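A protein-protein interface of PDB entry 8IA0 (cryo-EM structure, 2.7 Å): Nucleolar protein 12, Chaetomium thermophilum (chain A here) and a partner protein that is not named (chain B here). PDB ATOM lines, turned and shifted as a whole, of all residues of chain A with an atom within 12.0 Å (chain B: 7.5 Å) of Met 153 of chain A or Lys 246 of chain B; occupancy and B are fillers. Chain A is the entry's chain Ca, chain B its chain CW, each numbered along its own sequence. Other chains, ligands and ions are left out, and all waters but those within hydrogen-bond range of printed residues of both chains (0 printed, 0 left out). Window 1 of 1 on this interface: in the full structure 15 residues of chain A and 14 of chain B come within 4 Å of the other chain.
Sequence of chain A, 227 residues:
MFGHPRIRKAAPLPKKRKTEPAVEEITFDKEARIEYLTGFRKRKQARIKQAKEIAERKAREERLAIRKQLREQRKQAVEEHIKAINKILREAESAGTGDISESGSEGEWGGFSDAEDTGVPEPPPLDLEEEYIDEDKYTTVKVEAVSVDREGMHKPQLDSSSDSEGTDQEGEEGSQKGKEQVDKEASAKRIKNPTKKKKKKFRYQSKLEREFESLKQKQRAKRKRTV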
ATOM      1  N   THR A  97       7.628  22.848   9.672  1.00  0.00           N
ATOM      2  CA  THR A  97       8.128  23.744   8.637  1.00  0.00           C
ATOM      3  C   THR A  97       7.038  24.702   8.173  1.00  0.00           C
ATOM      4  O   THR A  97       6.011  24.857   8.835  1.00  0.00           O
ATOM      5  CB  THR A  97       8.666  22.961   7.424  1.00  0.00           C
ATOM      6  OG1 THR A  97       7.707  21.973   7.027  1.00  0.00           O
ATOM      7  CG2 THR A  97       9.979  22.276   7.770  1.00  0.00           C
ATOM      8  N   THR A 140      11.745  41.933  -4.052  1.00  0.00           N
ATOM      9  CA  THR A 140      11.046  40.656  -4.142  1.00  0.00           C
ATOM     10  C   THR A 140      11.926  39.516  -3.641  1.00  0.00           C
ATOM     11  O   THR A 140      12.952  39.200  -4.243  1.00  0.00           O
ATOM     12  CB  THR A 140      10.603  40.356  -5.584  1.00  0.00           C
ATOM     13  OG1 THR A 140      11.757  40.220  -6.422  1.00  0.00           O
ATOM     14  CG2 THR A 140       9.726  41.479  -6.117  1.00  0.00           C
ATOM     15  N   VAL A 141      11.518  38.901  -2.533  1.00  0.00           N
ATOM     16  CA  VAL A 141      12.263  37.810  -1.922  1.00  0.00           C
ATOM     17  C   VAL A 141      11.330  36.626  -1.716  1.00  0.00           C
ATOM     18  O   VAL A 141      10.119  36.784  -1.536  1.00  0.00           O
ATOM     19  CB  VAL A 141      12.910  38.232  -0.584  1.00  0.00           C
ATOM     20  CG1 VAL A 141      13.888  39.375  -0.800  1.00  0.00           C
ATOM     21  CG2 VAL A 141      11.843  38.624   0.427  1.00  0.00           C
ATOM     22  N   LYS A 142      11.907  35.428  -1.752  1.00  0.00           N
ATOM     23  CA  LYS A 142      11.189  34.187  -1.497  1.00  0.00           C
ATOM     24  C   LYS A 142      11.838  33.480  -0.318  1.00  0.00           C
ATOM     25  O   LYS A 142      13.060  33.297  -0.299  1.00  0.00           O
ATOM     26  CB  LYS A 142      11.190  33.273  -2.727  1.00  0.00           C
ATOM     27  CG  LYS A 142      10.962  33.984  -4.054  1.00  0.00           C
ATOM     28  CD  LYS A 142       9.654  34.759  -4.061  1.00  0.00           C
ATOM     29  CE  LYS A 142       9.623  35.776  -5.189  1.00  0.00           C
ATOM     30  NZ  LYS A 142      10.604  36.874  -4.974  1.00  0.00           N
ATOM     31  N   VAL A 143      11.026  33.086   0.660  1.00  0.00           N
ATOM     32  CA  VAL A 143      11.511  32.412   1.859  1.00  0.00           C
ATOM     33  C   VAL A 143      10.617  31.207   2.135  1.00  0.00           C
ATOM     34  O   VAL A 143       9.525  31.347   2.701  1.00  0.00           O
ATOM     35  CB  VAL A 143      11.572  33.363   3.069  1.00  0.00           C
ATOM     36  CG1 VAL A 143      10.285  34.187   3.203  1.00  0.00           C
ATOM     37  CG2 VAL A 143      11.878  32.596   4.351  1.00  0.00           C
ATOM     38  N   GLU A 144      11.072  30.028   1.718  1.00  0.00           N
ATOM     39  CA  GLU A 144      10.364  28.795   2.025  1.00  0.00           C
ATOM     40  C   GLU A 144      11.382  27.731   2.409  1.00  0.00           C
ATOM     41  O   GLU A 144      12.581  27.868   2.155  1.00  0.00           O
ATOM     42  CB  GLU A 144       9.486  28.300   0.860  1.00  0.00           C
ATOM     43  CG  GLU A 144      10.147  28.070  -0.520  1.00  0.00           C
ATOM     44  CD  GLU A 144      10.681  29.319  -1.220  1.00  0.00           C
ATOM     45  OE1 GLU A 144      10.934  30.348  -0.567  1.00  0.00           O
ATOM     46  OE2 GLU A 144      10.838  29.268  -2.459  1.00  0.00           O
ATOM     47  N   ALA A 145      10.883  26.670   3.031  1.00  0.00           N
ATOM     48  CA  ALA A 145      11.744  25.612   3.534  1.00  0.00           C
ATOM     49  C   ALA A 145      12.320  24.790   2.392  1.00  0.00           C
ATOM     50  O   ALA A 145      11.842  24.858   1.257  1.00  0.00           O
ATOM     51  CB  ALA A 145      10.969  24.704   4.486  1.00  0.00           C
ATOM     52  N   VAL A 146      13.354  24.004   2.703  1.00  0.00           N
ATOM     53  CA  VAL A 146      14.034  23.162   1.729  1.00  0.00           C
ATOM     54  C   VAL A 146      14.134  21.743   2.274  1.00  0.00           C
ATOM     55  O   VAL A 146      13.997  21.492   3.474  1.00  0.00           O
ATOM     56  CB  VAL A 146      15.445  23.683   1.387  1.00  0.00           C
ATOM     57  CG1 VAL A 146      15.389  25.073   0.805  1.00  0.00           C
ATOM     58  CG2 VAL A 146      16.339  23.633   2.613  1.00  0.00           C
ATOM     59  N   SER A 147      14.376  20.809   1.364  1.00  0.00           N
ATOM     60  CA  SER A 147      14.774  19.446   1.704  1.00  0.00           C
ATOM     61  C   SER A 147      15.910  19.084   0.757  1.00  0.00           C
ATOM     62  O   SER A 147      15.670  18.570  -0.340  1.00  0.00           O
ATOM     63  CB  SER A 147      13.605  18.477   1.588  1.00  0.00           C
ATOM     64  OG  SER A 147      12.655  18.709   2.612  1.00  0.00           O
ATOM     65  N   VAL A 148      17.141  19.359   1.176  1.00  0.00           N
ATOM     66  CA  VAL A 148      18.300  19.208   0.302  1.00  0.00           C
ATOM     67  C   VAL A 148      18.636  17.727   0.179  1.00  0.00           C
ATOM     68  O   VAL A 148      18.987  17.073   1.167  1.00  0.00           O
ATOM     69  CB  VAL A 148      19.495  20.009   0.833  1.00  0.00           C
ATOM     70  CG1 VAL A 148      20.792  19.521   0.208  1.00  0.00           C
ATOM     71  CG2 VAL A 148      19.291  21.497   0.574  1.00  0.00           C
ATOM     72  N   ASP A 149      18.522  17.195  -1.036  1.00  0.00           N
ATOM     73  CA  ASP A 149      18.838  15.798  -1.303  1.00  0.00           C
ATOM     74  C   ASP A 149      19.791  15.708  -2.486  1.00  0.00           C
ATOM     75  O   ASP A 149      20.140  16.735  -3.076  1.00  0.00           O
ATOM     76  CB  ASP A 149      17.564  14.996  -1.572  1.00  0.00           C
ATOM     77  CG  ASP A 149      16.651  14.928  -0.363  1.00  0.00           C
ATOM     78  OD1 ASP A 149      16.951  14.146   0.564  1.00  0.00           O
ATOM     79  OD2 ASP A 149      15.637  15.657  -0.338  1.00  0.00           O
ATOM     80  N   ARG A 150      20.189  14.485  -2.856  1.00  0.00           N
ATOM     81  CA  ARG A 150      21.223  14.304  -3.874  1.00  0.00           C
ATOM     82  C   ARG A 150      20.898  15.070  -5.151  1.00  0.00           C
ATOM     83  O   ARG A 150      21.783  15.688  -5.754  1.00  0.00           O
ATOM     84  CB  ARG A 150      21.400  12.817  -4.180  1.00  0.00           C
ATOM     85  CG  ARG A 150      22.093  12.024  -3.085  1.00  0.00           C
ATOM     86  CD  ARG A 150      23.544  12.445  -2.935  1.00  0.00           C
ATOM     87  NE  ARG A 150      24.326  11.458  -2.199  1.00  0.00           N
ATOM     88  CZ  ARG A 150      24.377  11.374  -0.877  1.00  0.00           C
ATOM     89  NH1 ARG A 150      23.701  12.208  -0.104  1.00  0.00           N
ATOM     90  NH2 ARG A 150      25.128  10.431  -0.316  1.00  0.00           N
ATOM     91  N   GLU A 151      19.634  15.043  -5.578  1.00  0.00           N
ATOM     92  CA  GLU A 151      19.233  15.838  -6.733  1.00  0.00           C
ATOM     93  C   GLU A 151      19.378  17.328  -6.454  1.00  0.00           C
ATOM     94  O   GLU A 151      19.846  18.086  -7.313  1.00  0.00           O
ATOM     95  CB  GLU A 151      17.798  15.495  -7.130  1.00  0.00           C
ATOM     96  CG  GLU A 151      17.437  14.033  -6.923  1.00  0.00           C
ATOM     97  CD  GLU A 151      16.679  13.790  -5.633  1.00  0.00           C
ATOM     98  OE1 GLU A 151      16.630  14.711  -4.790  1.00  0.00           O
ATOM     99  OE2 GLU A 151      16.133  12.681  -5.462  1.00  0.00           O
ATOM    100  N   GLY A 152      18.987  17.769  -5.261  1.00  0.00           N
ATOM    101  CA  GLY A 152      19.104  19.171  -4.910  1.00  0.00           C
ATOM    102  C   GLY A 152      17.984  19.686  -4.031  1.00  0.00           C
ATOM    103  O   GLY A 152      17.386  18.928  -3.262  1.00  0.00           O
ATOM    104  N   MET A 153      17.695  20.981  -4.137  1.00  0.00           N
ATOM    105  CA  MET A 153      16.660  21.600  -3.319  1.00  0.00           C
ATOM    106  C   MET A 153      15.288  21.100  -3.747  1.00  0.00           C
ATOM    107  O   MET A 153      14.884  21.288  -4.899  1.00  0.00           O
ATOM    108  CB  MET A 153      16.725  23.117  -3.444  1.00  0.00           C
ATOM    109  CG  MET A 153      17.806  23.777  -2.621  1.00  0.00           C
ATOM    110  SD  MET A 153      18.150  25.428  -3.251  1.00  0.00           S
ATOM    111  CE  MET A 153      19.467  25.929  -2.158  1.00  0.00           C
ATOM    112  N   HIS A 154      14.571  20.466  -2.825  1.00  0.00           N
ATOM    113  CA  HIS A 154      13.207  20.012  -3.063  1.00  0.00           C
ATOM    114  C   HIS A 154      12.307  20.599  -1.989  1.00  0.00           C
ATOM    115  O   HIS A 154      12.551  20.399  -0.796  1.00  0.00           O
ATOM    116  CB  HIS A 154      13.113  18.483  -3.059  1.00  0.00           C
ATOM    117  CG  HIS A 154      13.928  17.818  -4.124  1.00  0.00           C
ATOM    118  ND1 HIS A 154      14.586  18.521  -5.109  1.00  0.00           N
ATOM    119  CD2 HIS A 154      14.188  16.511  -4.359  1.00  0.00           C
ATOM    120  CE1 HIS A 154      15.218  17.676  -5.905  1.00  0.00           C
ATOM    121  NE2 HIS A 154      14.993  16.450  -5.471  1.00  0.00           N
ATOM    122  N   LYS A 155      11.276  21.319  -2.409  1.00  0.00           N
ATOM    123  CA  LYS A 155      10.304  21.855  -1.467  1.00  0.00           C
ATOM    124  C   LYS A 155       9.365  20.741  -1.025  1.00  0.00           C
ATOM    125  O   LYS A 155       8.741  20.098  -1.878  1.00  0.00           O
ATOM    126  CB  LYS A 155       9.518  22.995  -2.102  1.00  0.00           C
ATOM    127  CG  LYS A 155       8.145  23.228  -1.494  1.00  0.00           C
ATOM    128  CD  LYS A 155       7.259  24.034  -2.433  1.00  0.00           C
ATOM    129  CE  LYS A 155       5.785  23.762  -2.176  1.00  0.00           C
ATOM    130  NZ  LYS A 155       5.501  23.551  -0.730  1.00  0.00           N
ATOM    131  N   PRO A 156       9.242  20.468   0.282  1.00  0.00           N
ATOM    132  CA  PRO A 156       8.367  19.411   0.801  1.00  0.00           C
ATOM    133  C   PRO A 156       6.897  19.647   0.469  1.00  0.00           C
ATOM    134  O   PRO A 156       6.381  19.007  -0.447  1.00  0.00           O
ATOM    135  CB  PRO A 156       8.595  19.474   2.316  1.00  0.00           C
ATOM    136  CG  PRO A 156       9.890  20.190   2.487  1.00  0.00           C
ATOM    137  CD  PRO A 156       9.968  21.161   1.357  1.00  0.00           C
ATOM    138  N   ILE B  48      15.785  36.312   8.914  1.00  0.00           N
ATOM    139  CA  ILE B  48      15.803  34.858   8.933  1.00  0.00           C
ATOM    140  C   ILE B  48      17.048  34.311   9.621  1.00  0.00           C
ATOM    141  O   ILE B  48      16.964  33.324  10.350  1.00  0.00           O
ATOM    142  CB  ILE B  48      15.654  34.302   7.498  1.00  0.00           C
ATOM    143  CG1 ILE B  48      15.351  32.801   7.529  1.00  0.00           C
ATOM    144  CG2 ILE B  48      16.873  34.616   6.648  1.00  0.00           C
ATOM    145  CD1 ILE B  48      13.999  32.467   8.116  1.00  0.00           C
ATOM    146  N   ASP B  54      19.408  28.116   9.397  1.00  0.00           N
ATOM    147  CA  ASP B  54      20.460  28.084   8.392  1.00  0.00           C
ATOM    148  C   ASP B  54      19.911  28.592   7.071  1.00  0.00           C
ATOM    149  O   ASP B  54      18.866  28.135   6.603  1.00  0.00           O
ATOM    150  CB  ASP B  54      21.022  26.676   8.222  1.00  0.00           C
ATOM    151  CG  ASP B  54      21.266  25.994   9.539  1.00  0.00           C
ATOM    152  OD1 ASP B  54      22.260  26.333  10.207  1.00  0.00           O
ATOM    153  OD2 ASP B  54      20.452  25.138   9.923  1.00  0.00           O
ATOM    154  N   VAL B  55      20.614  29.546   6.475  1.00  0.00           N
ATOM    155  CA  VAL B  55      20.111  30.239   5.300  1.00  0.00           C
ATOM    156  C   VAL B  55      21.093  30.080   4.154  1.00  0.00           C
ATOM    157  O   VAL B  55      22.310  30.001   4.358  1.00  0.00           O
ATOM    158  CB  VAL B  55      19.842  31.730   5.585  1.00  0.00           C
ATOM    159  CG1 VAL B  55      18.987  31.869   6.828  1.00  0.00           C
ATOM    160  CG2 VAL B  55      21.139  32.500   5.724  1.00  0.00           C
ATOM    161  N   VAL B  56      20.549  29.998   2.946  1.00  0.00           N
ATOM    162  CA  VAL B  56      21.310  30.070   1.711  1.00  0.00           C
ATOM    163  C   VAL B  56      20.663  31.159   0.864  1.00  0.00           C
ATOM    164  O   VAL B  56      19.432  31.242   0.788  1.00  0.00           O
ATOM    165  CB  VAL B  56      21.353  28.705   0.991  1.00  0.00           C
ATOM    166  CG1 VAL B  56      20.119  28.470   0.147  1.00  0.00           C
ATOM    167  CG2 VAL B  56      22.601  28.589   0.155  1.00  0.00           C
ATOM    168  N   VAL B  57      21.479  32.043   0.300  1.00  0.00           N
ATOM    169  CA  VAL B  57      20.970  33.260  -0.318  1.00  0.00           C
ATOM    170  C   VAL B  57      21.333  33.276  -1.796  1.00  0.00           C
ATOM    171  O   VAL B  57      22.428  32.859  -2.187  1.00  0.00           O
ATOM    172  CB  VAL B  57      21.485  34.530   0.392  1.00  0.00           C
ATOM    173  CG1 VAL B  57      21.239  34.431   1.884  1.00  0.00           C
ATOM    174  CG2 VAL B  57      22.954  34.779   0.097  1.00  0.00           C
ATOM    175  N   GLU B  58      20.388  33.730  -2.616  1.00  0.00           N
ATOM    176  CA  GLU B  58      20.601  33.926  -4.048  1.00  0.00           C
ATOM    177  C   GLU B  58      20.644  35.433  -4.264  1.00  0.00           C
ATOM    178  O   GLU B  58      19.646  36.053  -4.632  1.00  0.00           O
ATOM    179  CB  GLU B  58      19.487  33.271  -4.856  1.00  0.00           C
ATOM    180  CG  GLU B  58      19.921  32.612  -6.158  1.00  0.00           C
ATOM    181  CD  GLU B  58      21.292  31.972  -6.081  1.00  0.00           C
ATOM    182  OE1 GLU B  58      21.559  31.246  -5.098  1.00  0.00           O
ATOM    183  OE2 GLU B  58      22.103  32.193  -7.005  1.00  0.00           O
ATOM    184  N   LEU B 224      25.473  30.015   3.783  1.00  0.00           N
ATOM    185  CA  LEU B 224      26.051  29.818   2.457  1.00  0.00           C
ATOM    186  C   LEU B 224      25.578  30.965   1.572  1.00  0.00           C
ATOM    187  O   LEU B 224      24.463  30.934   1.047  1.00  0.00           O
ATOM    188  CB  LEU B 224      25.640  28.463   1.889  1.00  0.00           C
ATOM    189  CG  LEU B 224      26.679  27.344   1.830  1.00  0.00           C
ATOM    190  CD1 LEU B 224      26.276  26.308   0.796  1.00  0.00           C
ATOM    191  CD2 LEU B 224      28.049  27.901   1.514  1.00  0.00           C
ATOM    192  N   LEU B 229      24.010  30.239  -7.380  1.00  0.00           N
ATOM    193  CA  LEU B 229      24.063  28.890  -6.820  1.00  0.00           C
ATOM    194  C   LEU B 229      23.205  27.926  -7.630  1.00  0.00           C
ATOM    195  O   LEU B 229      22.537  27.038  -7.093  1.00  0.00           O
ATOM    196  CB  LEU B 229      23.641  28.905  -5.355  1.00  0.00           C
ATOM    197  CG  LEU B 229      23.870  27.638  -4.527  1.00  0.00           C
ATOM    198  CD1 LEU B 229      25.343  27.276  -4.508  1.00  0.00           C
ATOM    199  CD2 LEU B 229      23.341  27.810  -3.127  1.00  0.00           C
ATOM    200  N   ALA B 232      26.109  24.660  -7.934  1.00  0.00           N
ATOM    201  CA  ALA B 232      26.526  23.826  -6.816  1.00  0.00           C
ATOM    202  C   ALA B 232      25.341  23.190  -6.103  1.00  0.00           C
ATOM    203  O   ALA B 232      25.471  22.797  -4.937  1.00  0.00           O
ATOM    204  CB  ALA B 232      27.369  24.629  -5.820  1.00  0.00           C
ATOM    205  N   VAL B 233      24.189  23.083  -6.768  1.00  0.00           N
ATOM    206  CA  VAL B 233      23.016  22.468  -6.166  1.00  0.00           C
ATOM    207  C   VAL B 233      23.247  20.990  -5.887  1.00  0.00           C
ATOM    208  O   VAL B 233      22.759  20.465  -4.881  1.00  0.00           O
ATOM    209  CB  VAL B 233      21.790  22.691  -7.080  1.00  0.00           C
ATOM    210  CG1 VAL B 233      22.107  22.287  -8.514  1.00  0.00           C
ATOM    211  CG2 VAL B 233      20.576  21.944  -6.558  1.00  0.00           C
ATOM    212  N   GLU B 234      24.001  20.306  -6.747  1.00  0.00           N
ATOM    213  CA  GLU B 234      24.282  18.888  -6.558  1.00  0.00           C
ATOM    214  C   GLU B 234      25.241  18.620  -5.405  1.00  0.00           C
ATOM    215  O   GLU B 234      25.332  17.476  -4.950  1.00  0.00           O
ATOM    216  CB  GLU B 234      24.863  18.294  -7.844  1.00  0.00           C
ATOM    217  CG  GLU B 234      23.924  18.327  -9.039  1.00  0.00           C
ATOM    218  CD  GLU B 234      22.765  17.359  -8.903  1.00  0.00           C
ATOM    219  OE1 GLU B 234      22.949  16.296  -8.274  1.00  0.00           O
ATOM    220  OE2 GLU B 234      21.675  17.658  -9.433  1.00  0.00           O
ATOM    221  N   LEU B 236      25.313  20.490  -2.369  1.00  0.00           N
ATOM    222  CA  LEU B 236      24.904  21.079  -1.099  1.00  0.00           C
ATOM    223  C   LEU B 236      24.804  20.044   0.010  1.00  0.00           C
ATOM    224  O   LEU B 236      24.688  20.414   1.183  1.00  0.00           O
ATOM    225  CB  LEU B 236      23.568  21.801  -1.260  1.00  0.00           C
ATOM    226  CG  LEU B 236      23.618  23.067  -2.112  1.00  0.00           C
ATOM    227  CD1 LEU B 236      22.262  23.739  -2.141  1.00  0.00           C
ATOM    228  CD2 LEU B 236      24.678  24.017  -1.586  1.00  0.00           C
ATOM    229  N   ILE B 237      24.840  18.757  -0.335  1.00  0.00           N
ATOM    230  CA  ILE B 237      24.757  17.705   0.673  1.00  0.00           C
ATOM    231  C   ILE B 237      25.995  17.732   1.559  1.00  0.00           C
ATOM    232  O   ILE B 237      25.921  17.479   2.767  1.00  0.00           O
ATOM    233  CB  ILE B 237      24.569  16.321   0.015  1.00  0.00           C
ATOM    234  CG1 ILE B 237      23.183  16.136  -0.625  1.00  0.00           C
ATOM    235  CG2 ILE B 237      24.787  15.209   1.022  1.00  0.00           C
ATOM    236  CD1 ILE B 237      22.760  17.173  -1.636  1.00  0.00           C
ATOM    237  N   MET B 241      23.374  21.002   5.897  1.00  0.00           N
ATOM    238  CA  MET B 241      22.617  21.911   6.744  1.00  0.00           C
ATOM    239  C   MET B 241      21.360  21.227   7.269  1.00  0.00           C
ATOM    240  O   MET B 241      20.620  20.578   6.524  1.00  0.00           O
ATOM    241  CB  MET B 241      22.234  23.167   5.963  1.00  0.00           C
ATOM    242  CG  MET B 241      23.327  23.700   5.058  1.00  0.00           C
ATOM    243  SD  MET B 241      22.691  24.795   3.776  1.00  0.00           S
ATOM    244  CE  MET B 241      21.893  23.614   2.690  1.00  0.00           C
ATOM    245  N   PRO B 244      17.477  24.053   6.749  1.00  0.00           N
ATOM    246  CA  PRO B 244      17.866  25.226   5.966  1.00  0.00           C
ATOM    247  C   PRO B 244      16.691  25.867   5.235  1.00  0.00           C
ATOM    248  O   PRO B 244      15.571  25.354   5.219  1.00  0.00           O
ATOM    249  CB  PRO B 244      18.885  24.653   4.967  1.00  0.00           C
ATOM    250  CG  PRO B 244      18.785  23.121   5.097  1.00  0.00           C
ATOM    251  CD  PRO B 244      17.586  22.830   5.944  1.00  0.00           C
ATOM    252  N   HIS B 245      16.976  27.016   4.619  1.00  0.00           N
ATOM    253  CA  HIS B 245      15.985  27.807   3.899  1.00  0.00           C
ATOM    254  C   HIS B 245      16.689  28.609   2.817  1.00  0.00           C
ATOM    255  O   HIS B 245      17.780  29.135   3.053  1.00  0.00           O
ATOM    256  CB  HIS B 245      15.258  28.772   4.842  1.00  0.00           C
ATOM    257  CG  HIS B 245      14.474  28.090   5.915  1.00  0.00           C
ATOM    258  ND1 HIS B 245      13.313  27.394   5.664  1.00  0.00           N
ATOM    259  CD2 HIS B 245      14.700  27.975   7.244  1.00  0.00           C
ATOM    260  CE1 HIS B 245      12.849  26.891   6.794  1.00  0.00           C
ATOM    261  NE2 HIS B 245      13.674  27.230   7.769  1.00  0.00           N
ATOM    262  N   LYS B 246      16.074  28.735   1.640  1.00  0.00           N
ATOM    263  CA  LYS B 246      16.677  29.544   0.587  1.00  0.00           C
ATOM    264  C   LYS B 246      16.092  30.950   0.630  1.00  0.00           C
ATOM    265  O   LYS B 246      14.903  31.126   0.916  1.00  0.00           O
ATOM    266  CB  LYS B 246      16.484  28.969  -0.820  1.00  0.00           C
ATOM    267  CG  LYS B 246      15.064  28.693  -1.291  1.00  0.00           C
ATOM    268  CD  LYS B 246      15.069  27.662  -2.411  1.00  0.00           C
ATOM    269  CE  LYS B 246      13.784  26.868  -2.469  1.00  0.00           C
ATOM    270  NZ  LYS B 246      13.351  26.319  -1.173  1.00  0.00           N
ATOM    271  N   ILE B 247      16.935  31.942   0.365  1.00  0.00           N
ATOM    272  CA  ILE B 247      16.521  33.327   0.182  1.00  0.00           C
ATOM    273  C   ILE B 247      16.977  33.750  -1.207  1.00  0.00           C
ATOM    274  O   ILE B 247      18.176  33.715  -1.505  1.00  0.00           O
ATOM    275  CB  ILE B 247      17.111  34.249   1.260  1.00  0.00           C
ATOM    276  CG1 ILE B 247      16.752  33.732   2.652  1.00  0.00           C
ATOM    277  CG2 ILE B 247      16.621  35.666   1.068  1.00  0.00           C
ATOM    278  CD1 ILE B 247      15.263  33.649   2.901  1.00  0.00           C
ATOM    279  N   THR B 248      16.029  34.127  -2.056  1.00  0.00           N
ATOM    280  CA  THR B 248      16.312  34.493  -3.436  1.00  0.00           C
ATOM    281  C   THR B 248      15.829  35.914  -3.680  1.00  0.00           C
ATOM    282  O   THR B 248      14.679  36.240  -3.374  1.00  0.00           O
ATOM    283  CB  THR B 248      15.627  33.531  -4.408  1.00  0.00           C
ATOM    284  OG1 THR B 248      14.226  33.494  -4.123  1.00  0.00           O
ATOM    285  CG2 THR B 248      16.187  32.131  -4.252  1.00  0.00           C
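O of Arg 150 of chain A lies close to OE1 of Glu 234 of chain B (2.8 Å).
O of Glu 151 of chain A sits close to OE2 of Glu 234 of chain B, at 2.8 Å.
The side-chain amino group of Lys 246 of chain B lies within hydrogen-bond range of the backbone carbonyl oxygen of Ala 145 of chain A, at 3.2 Å.
The backbone carbonyl oxygen of Lys 142 of chain A sits close to the backbone carbonyl oxygen of Lys 246 of chain B.
O of Thr 248 of chain B is in hydrogen-bond range of N of Lys 142 of chain A, 3.3 Å away.
The side-chain carboxylate of Glu 151 of chain A lies within hydrogen-bond range of a ring nitrogen (NE2) of His 154 of chain A (2.5 Å).
O of His 245 of chain B is in hydrogen-bond range of N of Val 56 of chain B (2.9 Å).
The backbone NH (N) of Glu 58 of chain B sits at hydrogen-bond distance from the backbone carbonyl oxygen (O) of Ile 247 of chain B.
The backbone carbonyl oxygen (O) of Val 56 of chain B sits at hydrogen-bond distance from the backbone NH (N) of Ile 247 of chain B, at 2.6 Å.
O of Gly 152 of chain A is in hydrogen-bond range of ND1 of His 154 of chain A (3.4 Å).
The backbone carbonyl oxygen of Thr 140 of chain A sits close to the side-chain amino group of Lys 142 of chain A, 3.4 Å away.
Among the printed residues, pairs that only touch across the chains: Asp 149 of chain A with Ile 237 of chain B, Val 146 of chain A with Lys 246 of chain B, Ala 145 of chain A with His 245 of chain B, Val 146 of chain A with Pro 244 of chain B, Val 141 of chain A with Thr 248 of chain B, Arg 150 of chain A with Ile 237 of chain B, Met 153 of chain A with Val 56 of chain B, Lys 142 of chain A with Ile 247 of chain B, Thr 140 of chain A with Thr 248 of chain B, Gly 152 of chain A with Val 233 of chain B, Met 153 of chain A with Leu 236 of chain B, Val 148 of chain A with Ile 237 of chain B, Glu 144 of chain A with His 245 of chain B, Glu 144 of chain A with Lys 246 of chain B, Val 143 of chain A with Ile 247 of chain B, Val 143 of chain A with Lys 246 of chain B, Val 148 of chain A with Leu 236 of chain B, Met 153 of chain A with Val 233 of chain B, Met 153 of chain A with Lys 246 of chain B, Val 148 of chain A with Met 241 of chain B, Val 146 of chain A with His 245 of chain B and Glu 151 of chain A with Val 233 of chain B.
Of chain B, only Val 56, Val 233, Leu 236 and Lys 246 come within 4 Å of Met 153 of chain A.
Lys 246 of chain B touches six residues of chain A.
Val 56 of chain B touches one residue of chain A.
Val 57 of chain B touches none of the printed residues of chain A.
Pro 244 of chain B touches just one residue of chain A: Val 146.
Ile 247 of chain B touches just these residues of chain A: Lys 142 (3.5 Å) and Val 143 (3.7 Å).
Thr 248 of chain B touches just these residues of chain A: Thr 140 (3.5 Å), Val 141 (3.2 Å) and Lys 142 (3.3 Å).
Printed residues of chain B within 4 Å of Arg 150 of chain A: Glu 234 (2.8 Å) and Ile 237 (3.4 Å).
Printed residues of chain A within 4 Å of Leu 236 of chain B: Val 148 and Met 153.
Printed residues of chain B within 4 Å of Gly 152 of chain A: Val 233 (3.5 Å).
Ser 147 of chain A touches none of the printed residues of chain B.
Leu 229 of chain B touches none of the printed residues of chain A.
The nearest residue of chain B that does not touch Met 153 of chain A is Leu 229 of chain B (4.4 Å).
Hydrophobic or aromatic side chains of chain A within 4 Å of the printed part of chain B: Val 141, Val 143, Ala 145, Val 146, Val 148 and Met 153.
Of the 19 printed residues of chain B, 11 touch a printed residue of chain A.
Hydrophobic or aromatic side chains of chain B that line the printed part of chain A: Val 56, Val 233, Leu 236, Ile 237, Met 241, Pro 244, His 245 and Ile 247.
Among the printed residues, 27 pairs touch across the chains.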
